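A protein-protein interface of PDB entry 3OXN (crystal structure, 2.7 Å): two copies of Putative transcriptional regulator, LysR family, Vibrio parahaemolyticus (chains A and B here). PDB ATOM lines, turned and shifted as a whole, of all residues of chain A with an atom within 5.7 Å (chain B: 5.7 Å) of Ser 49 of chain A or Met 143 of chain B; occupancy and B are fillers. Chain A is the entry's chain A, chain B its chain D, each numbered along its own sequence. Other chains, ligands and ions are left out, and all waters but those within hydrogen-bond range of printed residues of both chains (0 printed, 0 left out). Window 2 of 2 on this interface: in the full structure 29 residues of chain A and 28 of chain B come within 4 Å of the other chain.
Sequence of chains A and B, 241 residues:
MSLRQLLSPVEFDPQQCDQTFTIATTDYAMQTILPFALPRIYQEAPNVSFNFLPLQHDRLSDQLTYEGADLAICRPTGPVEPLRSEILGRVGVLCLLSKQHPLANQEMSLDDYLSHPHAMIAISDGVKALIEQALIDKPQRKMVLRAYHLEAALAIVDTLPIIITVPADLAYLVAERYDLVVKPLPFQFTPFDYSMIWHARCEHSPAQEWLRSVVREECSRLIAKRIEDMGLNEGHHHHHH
The side-chain hydroxyl (OH) of Tyr 42 of chain A is in hydrogen-bond range of the backbone carbonyl oxygen (O) of Val 144 of chain B. O of Met 143 of chain B lies within hydrogen-bond range of OG of Ser 49 of chain A, 2.7 Å away. N of Phe 50 of chain A is in hydrogen-bond range of O of Val 144 of chain B (2.7 Å). The backbone NH (N) of Arg 146 of chain B lies within hydrogen-bond range of the backbone carbonyl oxygen (O) of Phe 50 of chain A.
The backbone NH (N) of Ser 49 of chain A is in hydrogen-bond range of the backbone carbonyl oxygen (O) of Gln 19 of chain A, 3.4 Å away. The backbone NH (N) of Phe 21 of chain A sits at hydrogen-bond distance from the backbone carbonyl oxygen (O) of Ser 49 of chain A (2.9 Å). The backbone carbonyl oxygen (O) of Phe 21 of chain A is in hydrogen-bond range of the backbone NH (N) of Asn 51 of chain A (2.7 Å). OH of Tyr 42 of chain A lies close to N of Phe 50 of chain A, at 3.3 Å. The backbone carbonyl oxygen (O) of Lys 142 of chain B is in hydrogen-bond range of the backbone NH (N) of His 118 of chain B (2.7 Å). The backbone NH of Leu 145 of chain B sits at hydrogen-bond distance from the backbone carbonyl oxygen of His 118 of chain B, at 3.1 Å.
Among the printed residues, pairs that only touch across the chains: Asn 51 of chain A with Arg 146 of chain B (2.9 Å), Ser 49 of chain A with Val 144 of chain B (3.3 Å), Phe 50 of chain A with Leu 145 of chain B (3.4 Å) and Asn 47 of chain A with Lys 142 of chain B (3.8 Å).
Printed residues of chain B within 4 Å of Tyr 42 of chain A: Val 144. Printed residues of chain B within 4 Å of Asn 47 of chain A: Lys 142. Of the printed residues of chain B, Asn 51 of chain A touches Arg 146. Printed residues of chain A within 4 Å of Lys 142 of chain B: Asn 47. Of chain A, only Ser 49 comes within 4 Å of Met 143 of chain B. Of the printed residues of chain A, Val 144 of chain B touches Tyr 42, Ser 49 and Phe 50. The nearest residue of chain B that does not touch Ser 49 of chain A is Leu 145 of chain B (4.8 Å). The nearest residue of chain A that does not touch Met 143 of chain B is Phe 50 of chain A (5.2 Å). The nearest printed residue of chain A that does not touch Leu 145 of chain B is Tyr 42 of chain A (4.2 Å).
Printed residues of chain B that touch a printed residue of chain A: Lys 142, Met 143, Val 144, Leu 145 and Arg 146. Hydrophobic or aromatic side chains of chain A that line the printed part of chain B: Tyr 42 and Phe 50.
No position is printed for both chains. Of the 8 pairs that touch across the chains among the printed residues, none has its exchanged pair printed and touching as well.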
ATOM      1  N   ASP A  18      -2.749  13.562 -30.092  1.00  0.00           N
ATOM      2  CA  ASP A  18      -2.310  14.945 -30.239  1.00  0.00           C
ATOM      3  C   ASP A  18      -3.322  15.842 -29.541  1.00  0.00           C
ATOM      4  O   ASP A  18      -3.322  17.069 -29.673  1.00  0.00           O
ATOM      5  CB  ASP A  18      -2.171  15.317 -31.715  1.00  0.00           C
ATOM      6  CG  ASP A  18      -3.510  15.404 -32.428  1.00  0.00           C
ATOM      7  OD1 ASP A  18      -4.552  15.533 -31.744  1.00  0.00           O
ATOM      8  OD2 ASP A  18      -3.519  15.356 -33.681  1.00  0.00           O
ATOM      9  N   GLN A  19      -4.203  15.188 -28.801  1.00  0.00           N
ATOM     10  CA  GLN A  19      -5.252  15.848 -28.064  1.00  0.00           C
ATOM     11  C   GLN A  19      -4.672  16.646 -26.918  1.00  0.00           C
ATOM     12  O   GLN A  19      -3.656  16.286 -26.347  1.00  0.00           O
ATOM     13  CB  GLN A  19      -6.188  14.780 -27.523  1.00  0.00           C
ATOM     14  CG  GLN A  19      -7.065  15.220 -26.379  1.00  0.00           C
ATOM     15  CD  GLN A  19      -8.034  14.132 -25.998  1.00  0.00           C
ATOM     16  OE1 GLN A  19      -8.217  13.157 -26.743  1.00  0.00           O
ATOM     17  NE2 GLN A  19      -8.670  14.288 -24.840  1.00  0.00           N
ATOM     18  N   THR A  20      -5.320  17.744 -26.572  1.00  0.00           N
ATOM     19  CA  THR A  20      -4.855  18.519 -25.426  1.00  0.00           C
ATOM     20  C   THR A  20      -5.633  18.220 -24.126  1.00  0.00           C
ATOM     21  O   THR A  20      -6.834  17.953 -24.128  1.00  0.00           O
ATOM     22  CB  THR A  20      -4.796  20.036 -25.724  1.00  0.00           C
ATOM     23  OG1 THR A  20      -5.222  20.750 -24.564  1.00  0.00           O
ATOM     24  CG2 THR A  20      -5.694  20.388 -26.893  1.00  0.00           C
ATOM     25  N   PHE A  21      -4.922  18.243 -23.011  1.00  0.00           N
ATOM     26  CA  PHE A  21      -5.532  17.920 -21.743  1.00  0.00           C
ATOM     27  C   PHE A  21      -5.519  19.164 -20.888  1.00  0.00           C
ATOM     28  O   PHE A  21      -4.513  19.872 -20.819  1.00  0.00           O
ATOM     29  CB  PHE A  21      -4.774  16.778 -21.056  1.00  0.00           C
ATOM     30  CG  PHE A  21      -4.671  15.528 -21.898  1.00  0.00           C
ATOM     31  CD1 PHE A  21      -3.708  15.421 -22.893  1.00  0.00           C
ATOM     32  CD2 PHE A  21      -5.546  14.478 -21.710  1.00  0.00           C
ATOM     33  CE1 PHE A  21      -3.623  14.297 -23.678  1.00  0.00           C
ATOM     34  CE2 PHE A  21      -5.459  13.348 -22.497  1.00  0.00           C
ATOM     35  CZ  PHE A  21      -4.492  13.263 -23.484  1.00  0.00           C
ATOM     36  N   TYR A  42       5.527  13.494 -22.231  1.00  0.00           N
ATOM     37  CA  TYR A  42       5.830  13.956 -23.578  1.00  0.00           C
ATOM     38  C   TYR A  42       6.719  12.983 -24.318  1.00  0.00           C
ATOM     39  O   TYR A  42       6.669  12.873 -25.547  1.00  0.00           O
ATOM     40  CB  TYR A  42       6.485  15.330 -23.529  1.00  0.00           C
ATOM     41  CG  TYR A  42       5.464  16.426 -23.469  1.00  0.00           C
ATOM     42  CD1 TYR A  42       4.807  16.834 -24.617  1.00  0.00           C
ATOM     43  CD2 TYR A  42       5.123  17.027 -22.261  1.00  0.00           C
ATOM     44  CE1 TYR A  42       3.865  17.817 -24.575  1.00  0.00           C
ATOM     45  CE2 TYR A  42       4.182  18.018 -22.207  1.00  0.00           C
ATOM     46  CZ  TYR A  42       3.550  18.415 -23.373  1.00  0.00           C
ATOM     47  OH  TYR A  42       2.601  19.420 -23.355  1.00  0.00           O
ATOM     48  N   ALA A  45       4.185  10.452 -25.354  1.00  0.00           N
ATOM     49  CA  ALA A  45       3.129  10.931 -26.249  1.00  0.00           C
ATOM     50  C   ALA A  45       3.491  12.271 -26.888  1.00  0.00           C
ATOM     51  O   ALA A  45       2.833  13.280 -26.630  1.00  0.00           O
ATOM     52  CB  ALA A  45       1.825  11.053 -25.490  1.00  0.00           C
ATOM     53  N   ASN A  47       3.053  14.113 -29.457  1.00  0.00           N
ATOM     54  CA  ASN A  47       2.102  15.062 -30.047  1.00  0.00           C
ATOM     55  C   ASN A  47       1.223  15.755 -29.022  1.00  0.00           C
ATOM     56  O   ASN A  47       0.577  16.759 -29.319  1.00  0.00           O
ATOM     57  CB  ASN A  47       1.186  14.356 -31.041  1.00  0.00           C
ATOM     58  CG  ASN A  47       1.886  14.000 -32.327  1.00  0.00           C
ATOM     59  OD1 ASN A  47       1.341  14.212 -33.418  1.00  0.00           O
ATOM     60  ND2 ASN A  47       3.105  13.451 -32.213  1.00  0.00           N
ATOM     61  N   VAL A  48       1.191  15.190 -27.823  1.00  0.00           N
ATOM     62  CA  VAL A  48       0.260  15.589 -26.779  1.00  0.00           C
ATOM     63  C   VAL A  48       0.471  17.059 -26.413  1.00  0.00           C
ATOM     64  O   VAL A  48       1.571  17.593 -26.586  1.00  0.00           O
ATOM     65  CB  VAL A  48       0.437  14.667 -25.542  1.00  0.00           C
ATOM     66  CG1 VAL A  48       1.367  15.305 -24.505  1.00  0.00           C
ATOM     67  CG2 VAL A  48      -0.898  14.323 -24.940  1.00  0.00           C
ATOM     68  N   SER A  49      -0.588  17.705 -25.925  1.00  0.00           N
ATOM     69  CA  SER A  49      -0.569  19.129 -25.581  1.00  0.00           C
ATOM     70  C   SER A  49      -1.217  19.386 -24.204  1.00  0.00           C
ATOM     71  O   SER A  49      -2.252  18.803 -23.879  1.00  0.00           O
ATOM     72  CB  SER A  49      -1.300  19.905 -26.670  1.00  0.00           C
ATOM     73  OG  SER A  49      -1.329  21.296 -26.413  1.00  0.00           O
ATOM     74  N   PHE A  50      -0.619  20.260 -23.399  1.00  0.00           N
ATOM     75  CA  PHE A  50      -1.104  20.484 -22.033  1.00  0.00           C
ATOM     76  C   PHE A  50      -1.613  21.885 -21.694  1.00  0.00           C
ATOM     77  O   PHE A  50      -1.043  22.899 -22.095  1.00  0.00           O
ATOM     78  CB  PHE A  50      -0.027  20.101 -21.027  1.00  0.00           C
ATOM     79  CG  PHE A  50      -0.084  18.677 -20.613  1.00  0.00           C
ATOM     80  CD1 PHE A  50      -0.988  18.265 -19.656  1.00  0.00           C
ATOM     81  CD2 PHE A  50       0.752  17.750 -21.182  1.00  0.00           C
ATOM     82  CE1 PHE A  50      -1.051  16.956 -19.265  1.00  0.00           C
ATOM     83  CE2 PHE A  50       0.689  16.443 -20.806  1.00  0.00           C
ATOM     84  CZ  PHE A  50      -0.212  16.043 -19.839  1.00  0.00           C
ATOM     85  N   ASN A  51      -2.684  21.922 -20.916  1.00  0.00           N
ATOM     86  CA  ASN A  51      -3.215  23.181 -20.437  1.00  0.00           C
ATOM     87  C   ASN A  51      -3.441  23.190 -18.927  1.00  0.00           C
ATOM     88  O   ASN A  51      -4.451  22.689 -18.437  1.00  0.00           O
ATOM     89  CB  ASN A  51      -4.508  23.537 -21.158  1.00  0.00           C
ATOM     90  CG  ASN A  51      -4.821  25.010 -21.065  1.00  0.00           C
ATOM     91  OD1 ASN A  51      -3.916  25.826 -20.926  1.00  0.00           O
ATOM     92  ND2 ASN A  51      -6.098  25.363 -21.134  1.00  0.00           N
ATOM     93  N   HIS B 118       5.726  25.237 -28.620  1.00  0.00           N
ATOM     94  CA  HIS B 118       5.638  26.354 -27.707  1.00  0.00           C
ATOM     95  C   HIS B 118       5.136  25.950 -26.358  1.00  0.00           C
ATOM     96  O   HIS B 118       4.172  25.197 -26.241  1.00  0.00           O
ATOM     97  CB  HIS B 118       4.762  27.473 -28.275  1.00  0.00           C
ATOM     98  CG  HIS B 118       5.410  28.218 -29.390  1.00  0.00           C
ATOM     99  ND1 HIS B 118       5.220  27.884 -30.713  1.00  0.00           N
ATOM    100  CD2 HIS B 118       6.270  29.262 -29.384  1.00  0.00           C
ATOM    101  CE1 HIS B 118       5.922  28.703 -31.474  1.00  0.00           C
ATOM    102  NE2 HIS B 118       6.571  29.548 -30.693  1.00  0.00           N
ATOM    103  N   ALA B 119       5.817  26.465 -25.347  1.00  0.00           N
ATOM    104  CA  ALA B 119       5.297  26.498 -23.998  1.00  0.00           C
ATOM    105  C   ALA B 119       4.886  27.949 -23.681  1.00  0.00           C
ATOM    106  O   ALA B 119       5.685  28.881 -23.842  1.00  0.00           O
ATOM    107  CB  ALA B 119       6.344  25.993 -23.018  1.00  0.00           C
ATOM    108  N   MET B 120       3.638  28.145 -23.262  1.00  0.00           N
ATOM    109  CA  MET B 120       3.164  29.473 -22.862  1.00  0.00           C
ATOM    110  C   MET B 120       3.065  29.609 -21.339  1.00  0.00           C
ATOM    111  O   MET B 120       2.174  29.045 -20.701  1.00  0.00           O
ATOM    112  CB  MET B 120       1.819  29.783 -23.514  1.00  0.00           C
ATOM    113  CG  MET B 120       1.463  31.261 -23.523  1.00  0.00           C
ATOM    114  SD  MET B 120       0.207  31.731 -24.968  1.00  0.00           S
ATOM    115  CE  MET B 120       1.380  31.560 -26.528  1.00  0.00           C
ATOM    116  N   LYS B 128      -3.135  36.116 -24.256  1.00  0.00           N
ATOM    117  CA  LYS B 128      -3.028  34.996 -25.187  1.00  0.00           C
ATOM    118  C   LYS B 128      -3.762  35.369 -26.472  1.00  0.00           C
ATOM    119  O   LYS B 128      -3.244  35.193 -27.582  1.00  0.00           O
ATOM    120  CB  LYS B 128      -3.628  33.728 -24.549  1.00  0.00           C
ATOM    121  CG  LYS B 128      -3.187  32.406 -25.177  1.00  0.00           C
ATOM    122  CD  LYS B 128      -4.063  31.975 -26.350  1.00  0.00           C
ATOM    123  CE  LYS B 128      -3.341  30.975 -27.240  1.00  0.00           C
ATOM    124  NZ  LYS B 128      -2.393  31.640 -28.198  1.00  0.00           N
ATOM    125  N   ARG B 141       1.021  27.714 -34.994  1.00  0.00           N
ATOM    126  CA  ARG B 141       2.184  27.153 -34.318  1.00  0.00           C
ATOM    127  C   ARG B 141       1.702  26.059 -33.366  1.00  0.00           C
ATOM    128  O   ARG B 141       0.521  26.041 -32.999  1.00  0.00           O
ATOM    129  CB  ARG B 141       2.969  28.243 -33.572  1.00  0.00           C
ATOM    130  CG  ARG B 141       2.361  28.668 -32.233  1.00  0.00           C
ATOM    131  CD  ARG B 141       2.896  30.030 -31.746  1.00  0.00           C
ATOM    132  NE  ARG B 141       2.073  30.587 -30.674  1.00  0.00           N
ATOM    133  CZ  ARG B 141       0.857  31.086 -30.869  1.00  0.00           C
ATOM    134  NH1 ARG B 141       0.338  31.090 -32.088  1.00  0.00           N
ATOM    135  NH2 ARG B 141       0.152  31.570 -29.853  1.00  0.00           N
ATOM    136  N   LYS B 142       2.601  25.140 -32.995  1.00  0.00           N
ATOM    137  CA  LYS B 142       2.283  24.077 -32.033  1.00  0.00           C
ATOM    138  C   LYS B 142       2.365  24.564 -30.580  1.00  0.00           C
ATOM    139  O   LYS B 142       3.442  24.834 -30.038  1.00  0.00           O
ATOM    140  CB  LYS B 142       3.168  22.839 -32.243  1.00  0.00           C
ATOM    141  CG  LYS B 142       2.830  21.661 -31.302  1.00  0.00           C
ATOM    142  CD  LYS B 142       3.699  20.424 -31.564  1.00  0.00           C
ATOM    143  CE  LYS B 142       3.252  19.217 -30.734  1.00  0.00           C
ATOM    144  NZ  LYS B 142       4.208  18.063 -30.842  1.00  0.00           N
ATOM    145  N   MET B 143       1.199  24.689 -29.963  1.00  0.00           N
ATOM    146  CA  MET B 143       1.083  25.126 -28.584  1.00  0.00           C
ATOM    147  C   MET B 143       1.152  23.889 -27.726  1.00  0.00           C
ATOM    148  O   MET B 143       0.160  23.176 -27.578  1.00  0.00           O
ATOM    149  CB  MET B 143      -0.272  25.799 -28.391  1.00  0.00           C
ATOM    150  CG  MET B 143      -0.629  26.088 -26.951  1.00  0.00           C
ATOM    151  SD  MET B 143       0.489  27.520 -26.282  1.00  0.00           S
ATOM    152  CE  MET B 143       0.775  28.477 -27.965  1.00  0.00           C
ATOM    153  N   VAL B 144       2.315  23.611 -27.166  1.00  0.00           N
ATOM    154  CA  VAL B 144       2.507  22.322 -26.511  1.00  0.00           C
ATOM    155  C   VAL B 144       2.163  22.349 -25.024  1.00  0.00           C
ATOM    156  O   VAL B 144       1.626  21.392 -24.474  1.00  0.00           O
ATOM    157  CB  VAL B 144       3.928  21.789 -26.735  1.00  0.00           C
ATOM    158  CG1 VAL B 144       4.408  21.007 -25.534  1.00  0.00           C
ATOM    159  CG2 VAL B 144       3.984  20.948 -27.991  1.00  0.00           C
ATOM    160  N   LEU B 145       2.473  23.445 -24.365  1.00  0.00           N
ATOM    161  CA  LEU B 145       2.203  23.538 -22.953  1.00  0.00           C
ATOM    162  C   LEU B 145       1.704  24.921 -22.673  1.00  0.00           C
ATOM    163  O   LEU B 145       2.225  25.898 -23.204  1.00  0.00           O
ATOM    164  CB  LEU B 145       3.477  23.297 -22.148  1.00  0.00           C
ATOM    165  CG  LEU B 145       3.434  23.547 -20.641  1.00  0.00           C
ATOM    166  CD1 LEU B 145       2.766  22.402 -19.904  1.00  0.00           C
ATOM    167  CD2 LEU B 145       4.838  23.742 -20.114  1.00  0.00           C
ATOM    168  N   ARG B 146       0.685  25.010 -21.836  1.00  0.00           N
ATOM    169  CA  ARG B 146       0.238  26.297 -21.344  1.00  0.00           C
ATOM    170  C   ARG B 146       0.141  26.187 -19.819  1.00  0.00           C
ATOM    171  O   ARG B 146      -0.655  25.414 -19.288  1.00  0.00           O
ATOM    172  CB  ARG B 146      -1.097  26.663 -22.002  1.00  0.00           C
ATOM    173  CG  ARG B 146      -1.834  27.805 -21.344  1.00  0.00           C
ATOM    174  CD  ARG B 146      -1.448  29.146 -21.917  1.00  0.00           C
ATOM    175  NE  ARG B 146      -2.438  30.142 -21.531  1.00  0.00           N
ATOM    176  CZ  ARG B 146      -3.656  30.206 -22.057  1.00  0.00           C
ATOM    177  NH1 ARG B 146      -4.019  29.335 -22.987  1.00  0.00           N
ATOM    178  NH2 ARG B 146      -4.509  31.135 -21.652  1.00  0.00           N
